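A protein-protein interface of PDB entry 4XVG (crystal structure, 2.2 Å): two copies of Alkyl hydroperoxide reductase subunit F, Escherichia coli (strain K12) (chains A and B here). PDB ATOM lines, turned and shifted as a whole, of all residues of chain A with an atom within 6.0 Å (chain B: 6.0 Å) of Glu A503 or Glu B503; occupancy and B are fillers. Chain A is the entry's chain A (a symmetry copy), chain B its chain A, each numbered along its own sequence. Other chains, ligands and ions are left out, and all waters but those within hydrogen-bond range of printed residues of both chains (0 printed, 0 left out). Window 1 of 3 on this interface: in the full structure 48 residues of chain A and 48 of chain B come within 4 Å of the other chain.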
ATOM      1  N   ALA A 223     -25.651  -9.977 -20.404  1.00  0.00           N
ATOM      2  CA  ALA A 223     -25.941  -8.588 -20.732  1.00  0.00           C
ATOM      3  C   ALA A 223     -27.304  -8.143 -20.195  1.00  0.00           C
ATOM      4  O   ALA A 223     -27.414  -7.090 -19.541  1.00  0.00           O
ATOM      5  CB  ALA A 223     -25.873  -8.370 -22.235  1.00  0.00           C
ATOM      6  N   ILE A 472     -25.077   0.001 -32.743  1.00  0.00           N
ATOM      7  CA  ILE A 472     -25.162   0.900 -31.587  1.00  0.00           C
ATOM      8  C   ILE A 472     -24.043   1.939 -31.570  1.00  0.00           C
ATOM      9  O   ILE A 472     -23.001   1.753 -32.206  1.00  0.00           O
ATOM     10  CB  ILE A 472     -25.071   0.130 -30.255  1.00  0.00           C
ATOM     11  CG1 ILE A 472     -23.743  -0.636 -30.184  1.00  0.00           C
ATOM     12  CG2 ILE A 472     -26.296  -0.774 -30.069  1.00  0.00           C
ATOM     13  CD1 ILE A 472     -23.361  -1.139 -28.787  1.00  0.00           C
ATOM     14  N   CYS A 476     -24.713   2.797 -26.450  1.00  0.00           N
ATOM     15  CA  CYS A 476     -25.594   1.653 -26.682  1.00  0.00           C
ATOM     16  C   CYS A 476     -26.953   2.030 -27.288  1.00  0.00           C
ATOM     17  O   CYS A 476     -27.913   1.242 -27.209  1.00  0.00           O
ATOM     18  CB  CYS A 476     -25.774   0.840 -25.387  1.00  0.00           C
ATOM     19  SG  CYS A 476     -24.232   0.053 -24.856  1.00  0.00           S
ATOM     20  N   ALA A 485     -29.338  -1.383 -27.033  1.00  0.00           N
ATOM     21  CA  ALA A 485     -28.973  -2.783 -27.141  1.00  0.00           C
ATOM     22  C   ALA A 485     -27.618  -3.019 -26.493  1.00  0.00           C
ATOM     23  O   ALA A 485     -26.785  -2.106 -26.439  1.00  0.00           O
ATOM     24  CB  ALA A 485     -28.963  -3.216 -28.616  1.00  0.00           C
ATOM     25  N   ALA A 486     -27.397  -4.241 -26.009  1.00  0.00           N
ATOM     26  CA  ALA A 486     -26.156  -4.560 -25.335  1.00  0.00           C
ATOM     27  C   ALA A 486     -25.744  -6.019 -25.573  1.00  0.00           C
ATOM     28  O   ALA A 486     -26.602  -6.908 -25.642  1.00  0.00           O
ATOM     29  CB  ALA A 486     -26.308  -4.298 -23.840  1.00  0.00           C
ATOM     30  N   GLY A 487     -24.433  -6.263 -25.671  1.00  0.00           N
ATOM     31  CA  GLY A 487     -23.904  -7.618 -25.662  1.00  0.00           C
ATOM     32  C   GLY A 487     -23.733  -8.200 -27.061  1.00  0.00           C
ATOM     33  O   GLY A 487     -23.623  -7.459 -28.060  1.00  0.00           O
ATOM     34  N   THR A 490     -25.174  -7.018 -30.543  1.00  0.00           N
ATOM     35  CA  THR A 490     -24.835  -5.697 -31.095  1.00  0.00           C
ATOM     36  C   THR A 490     -23.566  -5.713 -31.936  1.00  0.00           C
ATOM     37  O   THR A 490     -22.961  -6.762 -32.148  1.00  0.00           O
ATOM     38  CB  THR A 490     -24.627  -4.670 -29.980  1.00  0.00           C
ATOM     39  OG1 THR A 490     -23.425  -5.001 -29.265  1.00  0.00           O
ATOM     40  CG2 THR A 490     -25.798  -4.687 -29.025  1.00  0.00           C
ATOM     41  N   VAL A 492     -20.806  -4.619 -30.989  1.00  0.00           N
ATOM     42  CA  VAL A 492     -19.637  -4.780 -30.132  1.00  0.00           C
ATOM     43  C   VAL A 492     -18.706  -5.818 -30.803  1.00  0.00           C
ATOM     44  O   VAL A 492     -19.161  -6.888 -31.231  1.00  0.00           O
ATOM     45  CB  VAL A 492     -20.052  -5.150 -28.695  1.00  0.00           C
ATOM     46  CG1 VAL A 492     -20.609  -6.606 -28.619  1.00  0.00           C
ATOM     47  CG2 VAL A 492     -18.898  -4.937 -27.719  1.00  0.00           C
ATOM     48  N   ILE A 498     -17.596 -10.944 -19.908  1.00  0.00           N
ATOM     49  CA  ILE A 498     -17.242  -9.722 -19.195  1.00  0.00           C
ATOM     50  C   ILE A 498     -17.497  -8.527 -20.096  1.00  0.00           C
ATOM     51  O   ILE A 498     -17.809  -7.421 -19.622  1.00  0.00           O
ATOM     52  CB  ILE A 498     -15.776  -9.754 -18.680  1.00  0.00           C
ATOM     53  CG1 ILE A 498     -15.550  -8.651 -17.645  1.00  0.00           C
ATOM     54  CG2 ILE A 498     -14.780  -9.692 -19.837  1.00  0.00           C
ATOM     55  CD1 ILE A 498     -16.155  -8.983 -16.279  1.00  0.00           C
ATOM     56  N   ILE A 499     -17.419  -8.764 -21.399  1.00  0.00           N
ATOM     57  CA  ILE A 499     -17.749  -7.724 -22.365  1.00  0.00           C
ATOM     58  C   ILE A 499     -19.267  -7.493 -22.407  1.00  0.00           C
ATOM     59  O   ILE A 499     -19.717  -6.346 -22.278  1.00  0.00           O
ATOM     60  CB  ILE A 499     -17.187  -8.057 -23.764  1.00  0.00           C
ATOM     61  CG1 ILE A 499     -15.658  -8.197 -23.659  1.00  0.00           C
ATOM     62  CG2 ILE A 499     -17.560  -6.964 -24.777  1.00  0.00           C
ATOM     63  CD1 ILE A 499     -14.968  -8.499 -24.980  1.00  0.00           C
ATOM     64  N   ALA A 500     -20.051  -8.569 -22.535  1.00  0.00           N
ATOM     65  CA  ALA A 500     -21.517  -8.443 -22.520  1.00  0.00           C
ATOM     66  C   ALA A 500     -22.007  -7.726 -21.262  1.00  0.00           C
ATOM     67  O   ALA A 500     -22.849  -6.823 -21.346  1.00  0.00           O
ATOM     68  CB  ALA A 500     -22.171  -9.809 -22.624  1.00  0.00           C
ATOM     69  N   THR A 501     -21.470  -8.118 -20.102  1.00  0.00           N
ATOM     70  CA  THR A 501     -21.911  -7.533 -18.839  1.00  0.00           C
ATOM     71  C   THR A 501     -21.573  -6.059 -18.747  1.00  0.00           C
ATOM     72  O   THR A 501     -22.376  -5.270 -18.242  1.00  0.00           O
ATOM     73  CB  THR A 501     -21.372  -8.276 -17.575  1.00  0.00           C
ATOM     74  OG1 THR A 501     -19.936  -8.338 -17.620  1.00  0.00           O
ATOM     75  CG2 THR A 501     -21.964  -9.682 -17.487  1.00  0.00           C
ATOM     76  N   GLY A 502     -20.395  -5.671 -19.221  1.00  0.00           N
ATOM     77  CA  GLY A 502     -20.052  -4.254 -19.225  1.00  0.00           C
ATOM     78  C   GLY A 502     -21.035  -3.471 -20.098  1.00  0.00           C
ATOM     79  O   GLY A 502     -21.472  -2.380 -19.723  1.00  0.00           O
ATOM     80  N   GLU A 503     -21.416  -4.038 -21.247  1.00  0.00           N
ATOM     81  CA  GLU A 503     -22.330  -3.349 -22.174  1.00  0.00           C
ATOM     82  C   GLU A 503     -23.745  -3.235 -21.610  1.00  0.00           C
ATOM     83  O   GLU A 503     -24.375  -2.179 -21.690  1.00  0.00           O
ATOM     84  CB  GLU A 503     -22.361  -4.087 -23.514  1.00  0.00           C
ATOM     85  CG  GLU A 503     -20.978  -4.240 -24.122  1.00  0.00           C
ATOM     86  CD  GLU A 503     -20.526  -2.978 -24.837  1.00  0.00           C
ATOM     87  OE1 GLU A 503     -19.377  -2.495 -24.590  1.00  0.00           O
ATOM     88  OE2 GLU A 503     -21.332  -2.488 -25.672  1.00  0.00           O
ATOM     89  N   GLY A 504     -24.241  -4.332 -21.040  1.00  0.00           N
ATOM     90  CA  GLY A 504     -25.522  -4.315 -20.368  1.00  0.00           C
ATOM     91  C   GLY A 504     -25.555  -3.219 -19.308  1.00  0.00           C
ATOM     92  O   GLY A 504     -26.575  -2.554 -19.142  1.00  0.00           O
ATOM     93  N   ALA A 505     -24.454  -3.012 -18.592  1.00  0.00           N
ATOM     94  CA  ALA A 505     -24.420  -1.933 -17.597  1.00  0.00           C
ATOM     95  C   ALA A 505     -24.429  -0.554 -18.270  1.00  0.00           C
ATOM     96  O   ALA A 505     -25.088   0.370 -17.772  1.00  0.00           O
ATOM     97  CB  ALA A 505     -23.213  -2.075 -16.678  1.00  0.00           C
ATOM     98  N   LYS A 506     -23.718  -0.404 -19.396  1.00  0.00           N
ATOM     99  CA  LYS A 506     -23.732   0.885 -20.123  1.00  0.00           C
ATOM    100  C   LYS A 506     -25.118   1.196 -20.668  1.00  0.00           C
ATOM    101  O   LYS A 506     -25.596   2.343 -20.591  1.00  0.00           O
ATOM    102  CB  LYS A 506     -22.735   0.900 -21.293  1.00  0.00           C
ATOM    103  CG  LYS A 506     -21.287   1.144 -20.883  1.00  0.00           C
ATOM    104  CD  LYS A 506     -20.383   1.412 -22.102  1.00  0.00           C
ATOM    105  CE  LYS A 506     -20.195   0.175 -22.958  1.00  0.00           C
ATOM    106  NZ  LYS A 506     -19.117   0.364 -23.974  1.00  0.00           N
ATOM    107  N   ALA A 507     -25.748   0.173 -21.239  1.00  0.00           N
ATOM    108  CA  ALA A 507     -27.046   0.323 -21.883  1.00  0.00           C
ATOM    109  C   ALA A 507     -28.068   0.760 -20.849  1.00  0.00           C
ATOM    110  O   ALA A 507     -28.924   1.615 -21.110  1.00  0.00           O
ATOM    111  CB  ALA A 507     -27.465  -1.008 -22.497  1.00  0.00           C
ATOM    112  N   SER A 508     -27.972   0.163 -19.666  1.00  0.00           N
ATOM    113  CA  SER A 508     -28.881   0.497 -18.583  1.00  0.00           C
ATOM    114  C   SER A 508     -28.697   1.933 -18.105  1.00  0.00           C
ATOM    115  O   SER A 508     -29.679   2.644 -17.862  1.00  0.00           O
ATOM    116  CB  SER A 508     -28.711  -0.483 -17.419  1.00  0.00           C
ATOM    117  OG  SER A 508     -29.406   0.015 -16.285  1.00  0.00           O
ATOM    118  N   ALA B 223      -9.495  -2.121 -15.347  1.00  0.00           N
ATOM    119  CA  ALA B 223      -9.313  -2.144 -16.792  1.00  0.00           C
ATOM    120  C   ALA B 223      -7.942  -2.697 -17.190  1.00  0.00           C
ATOM    121  O   ALA B 223      -7.844  -3.592 -18.050  1.00  0.00           O
ATOM    122  CB  ALA B 223      -9.509  -0.755 -17.377  1.00  0.00           C
ATOM    123  N   ILE B 472     -11.607   7.179 -28.043  1.00  0.00           N
ATOM    124  CA  ILE B 472     -11.486   5.838 -28.625  1.00  0.00           C
ATOM    125  C   ILE B 472     -12.660   5.488 -29.537  1.00  0.00           C
ATOM    126  O   ILE B 472     -13.736   6.087 -29.438  1.00  0.00           O
ATOM    127  CB  ILE B 472     -11.429   4.746 -27.539  1.00  0.00           C
ATOM    128  CG1 ILE B 472     -12.699   4.795 -26.680  1.00  0.00           C
ATOM    129  CG2 ILE B 472     -10.141   4.872 -26.714  1.00  0.00           C
ATOM    130  CD1 ILE B 472     -12.943   3.555 -25.812  1.00  0.00           C
ATOM    131  N   CYS B 476     -11.650   0.368 -29.123  1.00  0.00           N
ATOM    132  CA  CYS B 476     -10.724   0.938 -28.145  1.00  0.00           C
ATOM    133  C   CYS B 476      -9.440   1.507 -28.767  1.00  0.00           C
ATOM    134  O   CYS B 476      -8.432   1.690 -28.061  1.00  0.00           O
ATOM    135  CB  CYS B 476     -10.397  -0.091 -27.048  1.00  0.00           C
ATOM    136  SG  CYS B 476     -11.844  -0.492 -26.037  1.00  0.00           S
ATOM    137  N   ALA B 485      -6.845   2.280 -25.594  1.00  0.00           N
ATOM    138  CA  ALA B 485      -7.133   2.723 -24.243  1.00  0.00           C
ATOM    139  C   ALA B 485      -8.418   2.078 -23.747  1.00  0.00           C
ATOM    140  O   ALA B 485      -9.297   1.742 -24.550  1.00  0.00           O
ATOM    141  CB  ALA B 485      -7.231   4.256 -24.198  1.00  0.00           C
ATOM    142  N   ALA B 486      -8.528   1.913 -22.430  1.00  0.00           N
ATOM    143  CA  ALA B 486      -9.693   1.271 -21.857  1.00  0.00           C
ATOM    144  C   ALA B 486     -10.035   1.852 -20.477  1.00  0.00           C
ATOM    145  O   ALA B 486      -9.133   2.198 -19.704  1.00  0.00           O
ATOM    146  CB  ALA B 486      -9.442  -0.229 -21.743  1.00  0.00           C
ATOM    147  N   GLY B 487     -11.332   1.931 -20.166  1.00  0.00           N
ATOM    148  CA  GLY B 487     -11.778   2.240 -18.815  1.00  0.00           C
ATOM    149  C   GLY B 487     -12.021   3.729 -18.595  1.00  0.00           C
ATOM    150  O   GLY B 487     -12.251   4.495 -19.553  1.00  0.00           O
ATOM    151  N   THR B 490     -10.925   6.868 -20.725  1.00  0.00           N
ATOM    152  CA  THR B 490     -11.383   7.041 -22.113  1.00  0.00           C
ATOM    153  C   THR B 490     -12.710   7.781 -22.212  1.00  0.00           C
ATOM    154  O   THR B 490     -13.266   8.220 -21.207  1.00  0.00           O
ATOM    155  CB  THR B 490     -11.565   5.689 -22.805  1.00  0.00           C
ATOM    156  OG1 THR B 490     -12.686   5.013 -22.213  1.00  0.00           O
ATOM    157  CG2 THR B 490     -10.325   4.841 -22.638  1.00  0.00           C
ATOM    158  N   VAL B 492     -15.449   6.423 -22.815  1.00  0.00           N
ATOM    159  CA  VAL B 492     -16.537   5.568 -22.354  1.00  0.00           C
ATOM    160  C   VAL B 492     -17.453   6.427 -21.451  1.00  0.00           C
ATOM    161  O   VAL B 492     -16.971   7.143 -20.562  1.00  0.00           O
ATOM    162  CB  VAL B 492     -15.991   4.302 -21.666  1.00  0.00           C
ATOM    163  CG1 VAL B 492     -15.345   4.636 -20.286  1.00  0.00           C
ATOM    164  CG2 VAL B 492     -17.077   3.238 -21.537  1.00  0.00           C
ATOM    165  N   ILE B 498     -17.416  -2.829 -13.669  1.00  0.00           N
ATOM    166  CA  ILE B 498     -17.786  -3.851 -14.641  1.00  0.00           C
ATOM    167  C   ILE B 498     -17.672  -3.275 -16.041  1.00  0.00           C
ATOM    168  O   ILE B 498     -17.390  -3.998 -17.012  1.00  0.00           O
ATOM    169  CB  ILE B 498     -19.203  -4.427 -14.367  1.00  0.00           C
ATOM    170  CG1 ILE B 498     -19.414  -5.722 -15.152  1.00  0.00           C
ATOM    171  CG2 ILE B 498     -20.287  -3.386 -14.642  1.00  0.00           C
ATOM    172  CD1 ILE B 498     -18.687  -6.918 -14.533  1.00  0.00           C
ATOM    173  N   ILE B 499     -17.836  -1.962 -16.135  1.00  0.00           N
ATOM    174  CA  ILE B 499     -17.643  -1.277 -17.408  1.00  0.00           C
ATOM    175  C   ILE B 499     -16.150  -1.207 -17.758  1.00  0.00           C
ATOM    176  O   ILE B 499     -15.760  -1.600 -18.866  1.00  0.00           O
ATOM    177  CB  ILE B 499     -18.291   0.124 -17.396  1.00  0.00           C
ATOM    178  CG1 ILE B 499     -19.796  -0.032 -17.117  1.00  0.00           C
ATOM    179  CG2 ILE B 499     -18.063   0.842 -18.735  1.00  0.00           C
ATOM    180  CD1 ILE B 499     -20.567   1.279 -17.106  1.00  0.00           C
ATOM    181  N   ALA B 500     -15.316  -0.760 -16.812  1.00  0.00           N
ATOM    182  CA  ALA B 500     -13.863  -0.720 -17.043  1.00  0.00           C
ATOM    183  C   ALA B 500     -13.321  -2.088 -17.455  1.00  0.00           C
ATOM    184  O   ALA B 500     -12.543  -2.190 -18.412  1.00  0.00           O
ATOM    185  CB  ALA B 500     -13.139  -0.229 -15.802  1.00  0.00           C
ATOM    186  N   THR B 501     -13.743  -3.139 -16.742  1.00  0.00           N
ATOM    187  CA  THR B 501     -13.241  -4.481 -17.022  1.00  0.00           C
ATOM    188  C   THR B 501     -13.658  -4.969 -18.394  1.00  0.00           C
ATOM    189  O   THR B 501     -12.866  -5.612 -19.090  1.00  0.00           O
ATOM    190  CB  THR B 501     -13.637  -5.541 -15.945  1.00  0.00           C
ATOM    191  OG1 THR B 501     -15.065  -5.567 -15.785  1.00  0.00           O
ATOM    192  CG2 THR B 501     -12.957  -5.229 -14.611  1.00  0.00           C
ATOM    193  N   GLY B 502     -14.890  -4.682 -18.797  1.00  0.00           N
ATOM    194  CA  GLY B 502     -15.316  -5.063 -20.139  1.00  0.00           C
ATOM    195  C   GLY B 502     -14.451  -4.364 -21.190  1.00  0.00           C
ATOM    196  O   GLY B 502     -14.052  -4.980 -22.181  1.00  0.00           O
ATOM    197  N   GLU B 503     -14.126  -3.087 -20.962  1.00  0.00           N
ATOM    198  CA  GLU B 503     -13.328  -2.316 -21.931  1.00  0.00           C
ATOM    199  C   GLU B 503     -11.883  -2.805 -22.008  1.00  0.00           C
ATOM    200  O   GLU B 503     -11.326  -2.962 -23.096  1.00  0.00           O
ATOM    201  CB  GLU B 503     -13.357  -0.832 -21.560  1.00  0.00           C
ATOM    202  CG  GLU B 503     -14.772  -0.288 -21.460  1.00  0.00           C
ATOM    203  CD  GLU B 503     -15.351   0.051 -22.823  1.00  0.00           C
ATOM    204  OE1 GLU B 503     -16.505  -0.380 -23.138  1.00  0.00           O
ATOM    205  OE2 GLU B 503     -14.642   0.777 -23.568  1.00  0.00           O
ATOM    206  N   GLY B 504     -11.282  -3.043 -20.844  1.00  0.00           N
ATOM    207  CA  GLY B 504      -9.956  -3.621 -20.789  1.00  0.00           C
ATOM    208  C   GLY B 504      -9.906  -4.922 -21.581  1.00  0.00           C
ATOM    209  O   GLY B 504      -8.917  -5.193 -22.260  1.00  0.00           O
ATOM    210  N   ALA B 505     -10.959  -5.732 -21.515  1.00  0.00           N
ATOM    211  CA  ALA B 505     -10.980  -6.971 -22.303  1.00  0.00           C
ATOM    212  C   ALA B 505     -11.105  -6.676 -23.803  1.00  0.00           C
ATOM    213  O   ALA B 505     -10.466  -7.355 -24.620  1.00  0.00           O
ATOM    214  CB  ALA B 505     -12.102  -7.892 -21.840  1.00  0.00           C
ATOM    215  N   LYS B 506     -11.908  -5.670 -24.177  1.00  0.00           N
ATOM    216  CA  LYS B 506     -12.027  -5.300 -25.605  1.00  0.00           C
ATOM    217  C   LYS B 506     -10.707  -4.772 -26.150  1.00  0.00           C
ATOM    218  O   LYS B 506     -10.294  -5.114 -27.273  1.00  0.00           O
ATOM    219  CB  LYS B 506     -13.109  -4.235 -25.839  1.00  0.00           C
ATOM    220  CG  LYS B 506     -14.534  -4.778 -25.859  1.00  0.00           C
ATOM    221  CD  LYS B 506     -15.544  -3.725 -26.355  1.00  0.00           C
ATOM    222  CE  LYS B 506     -15.723  -2.593 -25.364  1.00  0.00           C
ATOM    223  NZ  LYS B 506     -16.885  -1.725 -25.720  1.00  0.00           N
ATOM    224  N   ALA B 507     -10.063  -3.921 -25.356  1.00  0.00           N
ATOM    225  CA  ALA B 507      -8.830  -3.262 -25.763  1.00  0.00           C
ATOM    226  C   ALA B 507      -7.760  -4.311 -26.002  1.00  0.00           C
ATOM    227  O   ALA B 507      -6.978  -4.228 -26.958  1.00  0.00           O
ATOM    228  CB  ALA B 507      -8.381  -2.302 -24.666  1.00  0.00           C
ATOM    229  N   SER B 508      -7.729  -5.304 -25.120  1.00  0.00           N
ATOM    230  CA  SER B 508      -6.761  -6.381 -25.238  1.00  0.00           C
ATOM    231  C   SER B 508      -6.992  -7.222 -26.488  1.00  0.00           C
ATOM    232  O   SER B 508      -6.038  -7.582 -27.189  1.00  0.00           O
ATOM    233  CB  SER B 508      -6.782  -7.262 -23.986  1.00  0.00           C
ATOM    234  OG  SER B 508      -6.033  -8.442 -24.234  1.00  0.00           O
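Among the printed residues, pairs that only touch across the chains: Ile A498 with Gly B502, Gly A502 with Ile B498, Lys A506 with Lys B506, Ile A498 with Thr B501, Thr A501 with Ile B498, Ile A498 with Ile B498, Ile A498 with Ala B505, Ala A505 with Ile B498, Val A492 with Lys B506, Lys A506 with Val B492, Lys A506 with Ile B499, Ile A499 with Lys B506, Glu A503 with Glu B503, Ile A499 with Gly B502 and Gly A502 with Ile B499.
The side-chain carboxylate (OE1) of Glu B503 is in salt-bridge range of the side-chain amino group (NZ) of Lys B506.
The side-chain hydroxyl (OG1) of Thr A490 sits close to the backbone NH (N) of Val A492.
OG1 of Thr B490 sits close to N of Val B492, 3.2 Å away.
The side-chain hydroxyl of Thr A501 sits at hydrogen-bond distance from the backbone carbonyl oxygen of Ile A498.
The backbone carbonyl oxygen (O) of Ile B498 is in hydrogen-bond range of the side-chain hydroxyl (OG1) of Thr B501 (3.1 Å).
NZ of Lys A506 lies within salt-bridge range of OE1 of Glu A503 (2.9 Å).
Of chain B, only Glu B503 (3.9 Å) and Lys B506 (2.8 Å) come within 4 Å of Glu A503.
Glu B503 touches two residues of chain A.
Printed residues of chain B within 4 Å of Val A492: Lys B506.
Of the printed residues of chain B, Ile A499 touches Gly B502 (3.9 Å) and Lys B506 (3.8 Å).
Gly B487 touches none of the printed residues of chain A.
The nearest residue of chain B that does not touch Glu A503 is Ile B498 (5.8 Å).
The nearest residue of chain A that does not touch Glu B503 is Ile A498 (5.8 Å).
The nearest printed residue of chain B that does not touch Thr A501 is Thr B501 (5.9 Å).
Val A492 touches Lys B506, and with the chains exchanged Lys A506 touches Val B492.
Ile A498 touches Thr B501, and with the chains exchanged Thr A501 touches Ile B498.
Ile A498 touches Ala B505, and with the chains exchanged Ala A505 touches Ile B498.
Ile A499 touches Lys B506, and with the chains exchanged Lys A506 touches Ile B499.
Of the 17 pairs that touch across the chains among the printed residues, 17 have their exchanged pair printed and touching as well.
The side-chain amino group of Lys B506 is in salt-bridge range of the side-chain carboxylate of Glu A503 (2.8 Å).
OE1 of Glu B503 lies within salt-bridge range of NZ of Lys A506.
Of the 19 printed residues of chain A, 8 touch a printed residue of chain B.
Hydrophobic or aromatic side chains of chain A within 4 Å of the printed part of chain B: Val A492, Ile A498, Ile A499 and Ala A505.
Of the 19 printed residues of chain B, 8 touch a printed residue of chain A.
Hydrophobic or aromatic side chains of chain B that line the printed part of chain A: Val B492, Ile B498, Ile B499 and Ala B505.
Among the printed residues, 17 pairs touch across the chains.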
